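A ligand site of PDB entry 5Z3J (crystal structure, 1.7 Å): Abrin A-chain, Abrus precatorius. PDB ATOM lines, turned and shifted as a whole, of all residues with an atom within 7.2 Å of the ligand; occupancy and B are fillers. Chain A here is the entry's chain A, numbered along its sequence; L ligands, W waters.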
ATOM      1  N   GLY A  81     -22.920  39.300  -8.187  1.00  0.00           N
ATOM      2  CA  GLY A  81     -21.901  39.074  -9.197  1.00  0.00           C
ATOM      3  C   GLY A  81     -22.232  37.832 -10.001  1.00  0.00           C
ATOM      4  O   GLY A  81     -22.561  36.776  -9.433  1.00  0.00           O
ATOM      5  N   ILE A  82     -22.140  37.960 -11.322  1.00  0.00           N
ATOM      6  CA  ILE A  82     -22.567  36.913 -12.245  1.00  0.00           C
ATOM      7  C   ILE A  82     -21.418  36.537 -13.165  1.00  0.00           C
ATOM      8  O   ILE A  82     -20.711  37.404 -13.697  1.00  0.00           O
ATOM      9  CB  ILE A  82     -23.792  37.363 -13.053  1.00  0.00           C
ATOM     10  CG1 ILE A  82     -25.005  37.383 -12.145  1.00  0.00           C
ATOM     11  CG2 ILE A  82     -23.995  36.451 -14.259  1.00  0.00           C
ATOM     12  CD1 ILE A  82     -26.245  37.965 -12.769  1.00  0.00           C
ATOM     13  N   ASN A  86     -21.594  31.126 -17.616  1.00  0.00           N
ATOM     14  CA  ASN A  86     -22.693  30.217 -17.336  1.00  0.00           C
ATOM     15  C   ASN A  86     -23.869  30.935 -16.676  1.00  0.00           C
ATOM     16  O   ASN A  86     -24.827  30.269 -16.283  1.00  0.00           O
ATOM     17  CB  ASN A  86     -22.204  29.073 -16.439  1.00  0.00           C
ATOM     18  CG  ASN A  86     -21.484  29.561 -15.201  1.00  0.00           C
ATOM     19  OD1 ASN A  86     -21.599  30.728 -14.833  1.00  0.00           O
ATOM     20  ND2 ASN A  86     -20.738  28.679 -14.557  1.00  0.00           N
ATOM     21  N   ALA A  87     -23.830  32.266 -16.552  1.00  0.00           N
ATOM     22  CA  ALA A  87     -24.903  33.050 -15.969  1.00  0.00           C
ATOM     23  C   ALA A  87     -25.113  32.731 -14.493  1.00  0.00           C
ATOM     24  O   ALA A  87     -26.178  33.029 -13.942  1.00  0.00           O
ATOM     25  CB  ALA A  87     -26.216  32.868 -16.726  1.00  0.00           C
ATOM     26  N   TYR A  88     -24.117  32.146 -13.835  1.00  0.00           N
ATOM     27  CA  TYR A  88     -24.242  31.793 -12.439  1.00  0.00           C
ATOM     28  C   TYR A  88     -24.038  33.013 -11.546  1.00  0.00           C
ATOM     29  O   TYR A  88     -23.154  33.845 -11.794  1.00  0.00           O
ATOM     30  CB  TYR A  88     -23.214  30.728 -12.053  1.00  0.00           C
ATOM     31  CG  TYR A  88     -23.742  29.327 -12.203  1.00  0.00           C
ATOM     32  CD1 TYR A  88     -24.212  28.864 -13.427  1.00  0.00           C
ATOM     33  CD2 TYR A  88     -23.772  28.467 -11.111  1.00  0.00           C
ATOM     34  CE1 TYR A  88     -24.701  27.580 -13.554  1.00  0.00           C
ATOM     35  CE2 TYR A  88     -24.262  27.183 -11.238  1.00  0.00           C
ATOM     36  CZ  TYR A  88     -24.723  26.739 -12.455  1.00  0.00           C
ATOM     37  OH  TYR A  88     -25.205  25.455 -12.575  1.00  0.00           O
ATOM     38  N   VAL A  89     -24.870  33.119 -10.524  1.00  0.00           N
ATOM     39  CA  VAL A  89     -24.606  34.031  -9.415  1.00  0.00           C
ATOM     40  C   VAL A  89     -23.501  33.403  -8.573  1.00  0.00           C
ATOM     41  O   VAL A  89     -23.668  32.320  -8.006  1.00  0.00           O
ATOM     42  CB  VAL A  89     -25.871  34.283  -8.584  1.00  0.00           C
ATOM     43  CG1 VAL A  89     -25.558  35.212  -7.424  1.00  0.00           C
ATOM     44  CG2 VAL A  89     -26.975  34.849  -9.457  1.00  0.00           C
ATOM     45  N   VAL A  90     -22.361  34.072  -8.507  1.00  0.00           N
ATOM     46  CA  VAL A  90     -21.204  33.555  -7.776  1.00  0.00           C
ATOM     47  C   VAL A  90     -20.926  34.322  -6.495  1.00  0.00           C
ATOM     48  O   VAL A  90     -20.100  33.863  -5.686  1.00  0.00           O
ATOM     49  CB  VAL A  90     -19.933  33.540  -8.668  1.00  0.00           C
ATOM     50  CG1 VAL A  90     -20.136  32.579  -9.836  1.00  0.00           C
ATOM     51  CG2 VAL A  90     -19.595  34.931  -9.161  1.00  0.00           C
ATOM     52  N   LEU A 101     -19.964  32.287  -3.227  1.00  0.00           N
ATOM     53  CA  LEU A 101     -20.374  30.896  -3.105  1.00  0.00           C
ATOM     54  C   LEU A 101     -19.149  30.012  -2.919  1.00  0.00           C
ATOM     55  O   LEU A 101     -18.038  30.349  -3.346  1.00  0.00           O
ATOM     56  CB  LEU A 101     -21.177  30.447  -4.334  1.00  0.00           C
ATOM     57  CG  LEU A 101     -22.672  30.772  -4.364  1.00  0.00           C
ATOM     58  CD1 LEU A 101     -23.423  30.121  -3.208  1.00  0.00           C
ATOM     59  CD2 LEU A 101     -22.924  32.278  -4.359  1.00  0.00           C
ATOM     60  N   ASP A 103     -18.177  27.331  -4.236  1.00  0.00           N
ATOM     61  CA  ASP A 103     -17.568  26.846  -5.466  1.00  0.00           C
ATOM     62  C   ASP A 103     -17.423  27.948  -6.503  1.00  0.00           C
ATOM     63  O   ASP A 103     -17.376  27.674  -7.706  1.00  0.00           O
ATOM     64  CB  ASP A 103     -18.370  25.674  -6.034  1.00  0.00           C
ATOM     65  CG  ASP A 103     -19.829  26.007  -6.248  1.00  0.00           C
ATOM     66  OD1 ASP A 103     -20.292  27.073  -5.794  1.00  0.00           O
ATOM     67  OD2 ASP A 103     -20.516  25.172  -6.879  1.00  0.00           O
ATOM     68  N   TYR A 124     -22.229  25.448  -1.538  1.00  0.00           N
ATOM     69  CA  TYR A 124     -22.022  25.548  -2.967  1.00  0.00           C
ATOM     70  C   TYR A 124     -23.207  26.234  -3.623  1.00  0.00           C
ATOM     71  O   TYR A 124     -24.329  26.234  -3.114  1.00  0.00           O
ATOM     72  CB  TYR A 124     -21.820  24.158  -3.590  1.00  0.00           C
ATOM     73  CG  TYR A 124     -20.703  23.347  -2.972  1.00  0.00           C
ATOM     74  CD1 TYR A 124     -19.383  23.769  -3.057  1.00  0.00           C
ATOM     75  CD2 TYR A 124     -20.965  22.137  -2.337  1.00  0.00           C
ATOM     76  CE1 TYR A 124     -18.357  23.025  -2.503  1.00  0.00           C
ATOM     77  CE2 TYR A 124     -19.938  21.392  -1.783  1.00  0.00           C
ATOM     78  CZ  TYR A 124     -18.637  21.836  -1.877  1.00  0.00           C
ATOM     79  OH  TYR A 124     -17.618  21.092  -1.330  1.00  0.00           O
ATOM     80  N   GLY A 125     -22.952  26.825  -4.786  1.00  0.00           N
ATOM     81  CA  GLY A 125     -23.983  27.531  -5.515  1.00  0.00           C
ATOM     82  C   GLY A 125     -24.952  26.669  -6.282  1.00  0.00           C
ATOM     83  O   GLY A 125     -25.729  27.194  -7.079  1.00  0.00           O
ATOM     84  N   THR A 126     -24.945  25.360  -6.065  1.00  0.00           N
ATOM     85  CA  THR A 126     -25.841  24.473  -6.778  1.00  0.00           C
ATOM     86  C   THR A 126     -27.204  24.406  -6.090  1.00  0.00           C
ATOM     87  O   THR A 126     -27.327  24.628  -4.887  1.00  0.00           O
ATOM     88  CB  THR A 126     -25.242  23.068  -6.856  1.00  0.00           C
ATOM     89  OG1 THR A 126     -25.178  22.511  -5.535  1.00  0.00           O
ATOM     90  CG2 THR A 126     -23.857  23.096  -7.456  1.00  0.00           C
ATOM     91  N   TYR A 127     -28.232  24.073  -6.872  1.00  0.00           N
ATOM     92  CA  TYR A 127     -29.539  23.836  -6.258  1.00  0.00           C
ATOM     93  C   TYR A 127     -29.457  22.730  -5.228  1.00  0.00           C
ATOM     94  O   TYR A 127     -30.094  22.807  -4.169  1.00  0.00           O
ATOM     95  CB  TYR A 127     -30.572  23.489  -7.337  1.00  0.00           C
ATOM     96  CG  TYR A 127     -30.988  24.658  -8.205  1.00  0.00           C
ATOM     97  CD1 TYR A 127     -31.251  25.909  -7.655  1.00  0.00           C
ATOM     98  CD2 TYR A 127     -31.130  24.496  -9.569  1.00  0.00           C
ATOM     99  CE1 TYR A 127     -31.632  26.967  -8.452  1.00  0.00           C
ATOM    100  CE2 TYR A 127     -31.511  25.543 -10.379  1.00  0.00           C
ATOM    101  CZ  TYR A 127     -31.762  26.784  -9.814  1.00  0.00           C
ATOM    102  OH  TYR A 127     -32.143  27.832 -10.611  1.00  0.00           O
ATOM    103  N   GLY A 128     -28.664  21.687  -5.509  1.00  0.00           N
ATOM    104  CA  GLY A 128     -28.534  20.592  -4.562  1.00  0.00           C
ATOM    105  C   GLY A 128     -28.126  21.069  -3.185  1.00  0.00           C
ATOM    106  O   GLY A 128     -28.774  20.743  -2.176  1.00  0.00           O
ATOM    107  N   LEU A 130     -27.886  24.378  -2.116  1.00  0.00           N
ATOM    108  CA  LEU A 130     -28.747  25.456  -1.647  1.00  0.00           C
ATOM    109  C   LEU A 130     -30.043  24.894  -1.073  1.00  0.00           C
ATOM    110  O   LEU A 130     -30.488  25.325   0.002  1.00  0.00           O
ATOM    111  CB  LEU A 130     -29.051  26.429  -2.792  1.00  0.00           C
ATOM    112  CG  LEU A 130     -27.890  27.311  -3.281  1.00  0.00           C
ATOM    113  CD1 LEU A 130     -28.300  28.048  -4.530  1.00  0.00           C
ATOM    114  CD2 LEU A 130     -27.454  28.294  -2.205  1.00  0.00           C
ATOM    115  N   ARG A 138     -36.787  23.951  -4.485  1.00  0.00           N
ATOM    116  CA  ARG A 138     -37.276  25.038  -5.330  1.00  0.00           C
ATOM    117  C   ARG A 138     -38.804  25.023  -5.401  1.00  0.00           C
ATOM    118  O   ARG A 138     -39.438  26.077  -5.363  1.00  0.00           O
ATOM    119  CB  ARG A 138     -36.694  24.920  -6.735  1.00  0.00           C
ATOM    120  CG  ARG A 138     -35.249  25.367  -6.867  1.00  0.00           C
ATOM    121  CD  ARG A 138     -34.665  24.880  -8.182  1.00  0.00           C
ATOM    122  NE  ARG A 138     -34.320  23.468  -8.133  1.00  0.00           N
ATOM    123  CZ  ARG A 138     -34.073  22.706  -9.191  1.00  0.00           C
ATOM    124  NH1 ARG A 138     -34.159  23.220 -10.410  1.00  0.00           N
ATOM    125  NH2 ARG A 138     -33.747  21.432  -9.036  1.00  0.00           N
ATOM    126  N   LEU A 169     -30.866  33.023  -2.088  1.00  0.00           N
ATOM    127  CA  LEU A 169     -30.162  32.819  -3.351  1.00  0.00           C
ATOM    128  C   LEU A 169     -30.997  32.012  -4.336  1.00  0.00           C
ATOM    129  O   LEU A 169     -31.001  32.287  -5.533  1.00  0.00           O
ATOM    130  CB  LEU A 169     -28.811  32.147  -3.094  1.00  0.00           C
ATOM    131  CG  LEU A 169     -27.725  33.132  -2.649  1.00  0.00           C
ATOM    132  CD1 LEU A 169     -26.519  32.422  -2.041  1.00  0.00           C
ATOM    133  CD2 LEU A 169     -27.291  34.017  -3.814  1.00  0.00           C
ATOM    134  N   ILE A 172     -33.232  34.593  -5.946  1.00  0.00           N
ATOM    135  CA  ILE A 172     -32.529  35.492  -6.855  1.00  0.00           C
ATOM    136  C   ILE A 172     -32.073  34.750  -8.105  1.00  0.00           C
ATOM    137  O   ILE A 172     -32.252  35.217  -9.240  1.00  0.00           O
ATOM    138  CB  ILE A 172     -31.337  36.148  -6.141  1.00  0.00           C
ATOM    139  CG1 ILE A 172     -31.835  37.166  -5.098  1.00  0.00           C
ATOM    140  CG2 ILE A 172     -30.406  36.808  -7.136  1.00  0.00           C
ATOM    141  CD1 ILE A 172     -30.744  37.682  -4.160  1.00  0.00           C
ATOM    142  N   ILE A 173     -31.482  33.571  -7.918  1.00  0.00           N
ATOM    143  CA  ILE A 173     -30.979  32.790  -9.037  1.00  0.00           C
ATOM    144  C   ILE A 173     -32.079  32.562 -10.075  1.00  0.00           C
ATOM    145  O   ILE A 173     -31.862  32.703 -11.279  1.00  0.00           O
ATOM    146  CB  ILE A 173     -30.401  31.455  -8.545  1.00  0.00           C
ATOM    147  CG1 ILE A 173     -29.091  31.677  -7.797  1.00  0.00           C
ATOM    148  CG2 ILE A 173     -30.205  30.502  -9.715  1.00  0.00           C
ATOM    149  CD1 ILE A 173     -28.612  30.467  -7.018  1.00  0.00           C
ATOM    150  N   GLN A 174     -33.272  32.195  -9.613  1.00  0.00           N
ATOM    151  CA  GLN A 174     -34.329  31.867 -10.559  1.00  0.00           C
ATOM    152  C   GLN A 174     -34.931  33.117 -11.196  1.00  0.00           C
ATOM    153  O   GLN A 174     -35.248  33.112 -12.390  1.00  0.00           O
ATOM    154  CB  GLN A 174     -35.421  31.047  -9.873  1.00  0.00           C
ATOM    155  CG  GLN A 174     -34.981  29.628  -9.544  1.00  0.00           C
ATOM    156  CD  GLN A 174     -36.027  28.879  -8.760  1.00  0.00           C
ATOM    157  OE1 GLN A 174     -36.181  29.074  -7.557  1.00  0.00           O
ATOM    158  NE2 GLN A 174     -36.764  28.017  -9.441  1.00  0.00           N
ATOM    159  N   ALA A 177     -31.021  34.671 -13.110  1.00  0.00           N
ATOM    160  CA  ALA A 177     -30.270  33.813 -14.026  1.00  0.00           C
ATOM    161  C   ALA A 177     -31.202  32.934 -14.868  1.00  0.00           C
ATOM    162  O   ALA A 177     -31.113  32.925 -16.097  1.00  0.00           O
ATOM    163  CB  ALA A 177     -29.278  32.953 -13.240  1.00  0.00           C
ATOM    164  N   GLU A 178     -32.094  32.182 -14.214  1.00  0.00           N
ATOM    165  CA  GLU A 178     -32.973  31.301 -14.970  1.00  0.00           C
ATOM    166  C   GLU A 178     -33.902  32.098 -15.885  1.00  0.00           C
ATOM    167  O   GLU A 178     -34.186  31.681 -17.006  1.00  0.00           O
ATOM    168  CB  GLU A 178     -33.797  30.416 -14.030  1.00  0.00           C
ATOM    169  CG  GLU A 178     -32.963  29.528 -13.099  1.00  0.00           C
ATOM    170  CD  GLU A 178     -32.246  28.402 -13.832  1.00  0.00           C
ATOM    171  OE1 GLU A 178     -32.167  28.424 -15.077  1.00  0.00           O
ATOM    172  OE2 GLU A 178     -31.762  27.479 -13.137  1.00  0.00           O
ATOM    173  N   ARG A 181     -32.117  32.892 -18.948  1.00  0.00           N
ATOM    174  CA  ARG A 181     -31.915  31.751 -19.832  1.00  0.00           C
ATOM    175  C   ARG A 181     -33.183  31.383 -20.599  1.00  0.00           C
ATOM    176  O   ARG A 181     -33.114  30.987 -21.759  1.00  0.00           O
ATOM    177  CB  ARG A 181     -31.444  30.543 -19.031  1.00  0.00           C
ATOM    178  CG  ARG A 181     -30.087  30.683 -18.413  1.00  0.00           C
ATOM    179  CD  ARG A 181     -29.890  29.584 -17.407  1.00  0.00           C
ATOM    180  NE  ARG A 181     -28.579  29.629 -16.778  1.00  0.00           N
ATOM    181  CZ  ARG A 181     -28.328  29.281 -15.526  1.00  0.00           C
ATOM    182  NH1 ARG A 181     -29.305  28.857 -14.736  1.00  0.00           N
ATOM    183  NH2 ARG A 181     -27.093  29.367 -15.043  1.00  0.00           N
ATOM    184  N   GLU A 209     -34.903  24.322 -15.876  1.00  0.00           N
ATOM    185  CA  GLU A 209     -33.735  24.582 -15.050  1.00  0.00           C
ATOM    186  C   GLU A 209     -32.823  23.362 -15.000  1.00  0.00           C
ATOM    187  O   GLU A 209     -31.598  23.493 -15.065  1.00  0.00           O
ATOM    188  CB  GLU A 209     -34.167  24.987 -13.648  1.00  0.00           C
ATOM    189  CG  GLU A 209     -34.993  26.253 -13.599  1.00  0.00           C
ATOM    190  CD  GLU A 209     -35.484  26.563 -12.200  1.00  0.00           C
ATOM    191  OE1 GLU A 209     -35.308  25.692 -11.313  1.00  0.00           O
ATOM    192  OE2 GLU A 209     -36.028  27.657 -11.984  1.00  0.00           O
ATOM    193  N   TRP A 212     -30.919  22.772 -18.746  1.00  0.00           N
ATOM    194  CA  TRP A 212     -30.364  23.874 -19.521  1.00  0.00           C
ATOM    195  C   TRP A 212     -29.148  23.427 -20.315  1.00  0.00           C
ATOM    196  O   TRP A 212     -29.040  23.690 -21.522  1.00  0.00           O
ATOM    197  CB  TRP A 212     -30.018  25.030 -18.599  1.00  0.00           C
ATOM    198  CG  TRP A 212     -29.429  26.214 -19.293  1.00  0.00           C
ATOM    199  CD1 TRP A 212     -29.973  26.904 -20.338  1.00  0.00           C
ATOM    200  CD2 TRP A 212     -28.200  26.877 -18.968  1.00  0.00           C
ATOM    201  NE1 TRP A 212     -29.148  27.948 -20.698  1.00  0.00           N
ATOM    202  CE2 TRP A 212     -28.055  27.955 -19.869  1.00  0.00           C
ATOM    203  CE3 TRP A 212     -27.199  26.658 -18.009  1.00  0.00           C
ATOM    204  CZ2 TRP A 212     -26.959  28.809 -19.834  1.00  0.00           C
ATOM    205  CZ3 TRP A 212     -26.110  27.512 -17.982  1.00  0.00           C
ATOM    206  CH2 TRP A 212     -26.002  28.574 -18.891  1.00  0.00           C
HETATM  207  N1  LIG L   1     -28.407  27.937 -12.051  1.00  0.00           N
HETATM  208  C1  LIG L   1     -27.710  28.967 -11.529  1.00  0.00           C
HETATM  209  C2  LIG L   1     -27.139  28.827 -10.277  1.00  0.00           C
HETATM  210  C3  LIG L   1     -27.262  27.676  -9.577  1.00  0.00           C
HETATM  211  C4  LIG L   1     -27.952  26.645 -10.106  1.00  0.00           C
HETATM  212  C5  LIG L   1     -28.531  26.776 -11.351  1.00  0.00           C
HETATM  213  C6  LIG L   1     -26.359  29.992  -9.703  1.00  0.00           C
HETATM  214  O1  LIG L   1     -26.516  31.062 -10.188  1.00  0.00           O
HETATM  215  N2  LIG L   1     -25.434  29.787  -8.606  1.00  0.00           N
HETATM  216  O   HOH W   1     -30.058  25.256 -13.802  1.00  0.00           O
HETATM  217  O   HOH W   2     -22.427  29.914  -7.854  1.00  0.00           O
HETATM  218  O   HOH W   3     -27.806  23.217  -9.711  1.00  0.00           O
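Water W2 bridges the backbone carbonyl oxygen of Val 89 (2.7 Å) and a nitrogen (N2) of the ligand (3.1 Å). Water W1 lies within hydrogen-bond range of the backbone carbonyl oxygen (O) of Glu 209 (2.7 Å) and the side-chain carboxylate (OE2) of Glu 178 (2.9 Å).
The side-chain carboxylate (OD1) of Asp 103 sits at hydrogen-bond distance from the backbone NH (N) of Gly 125 (2.9 Å). NH1 of Arg 181 lies within salt-bridge range of OE1 of Glu 178 (2.9 Å). The backbone carbonyl oxygen of Asn 86 sits at hydrogen-bond distance from the guanidinium group of Arg 181, at 2.7 Å. N of Tyr 88 sits at hydrogen-bond distance from OD1 of Asn 86 (3.1 Å). OH of Tyr 127 sits at hydrogen-bond distance from OE2 of Glu 178 (2.6 Å). The backbone carbonyl oxygen (O) of Ile 173 sits at hydrogen-bond distance from the backbone NH (N) of Glu 178 (3.0 Å).
Tyr 88 touches the ligand (CA to O1, 3.3 Å). CE2 of Tyr 127 touches C5 of the ligand, 3.4 Å away. CG2 of Ile 173 touches C1 of the ligand, 3.4 Å away. Glu 178 touches the ligand (OE2 to N1, 3.6 Å). Hydrophobic or aromatic side chains within 4 Å of the ligand: Tyr 88, Val 89, Tyr 127 and Ile 173. Seven residues have an atom within 4 Å of the ligand: Tyr 88, Val 89, Gly 125, Tyr 127, Ile 173, Glu 178 and Arg 181. The nearest printed residue that does not touch the ligand is Ala 87 (4.3 Å).
N of Val 89 sits at hydrogen-bond distance from O1 of the ligand. N2 of the ligand sits at hydrogen-bond distance from O of Val 89 (3.1 Å). The backbone carbonyl oxygen (O) of Gly 125 lies close to a nitrogen (N2) of the ligand, at 3.0 Å. A nitrogen (N1) of the ligand sits at hydrogen-bond distance from the guanidinium group of Arg 181, at 3.0 Å.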
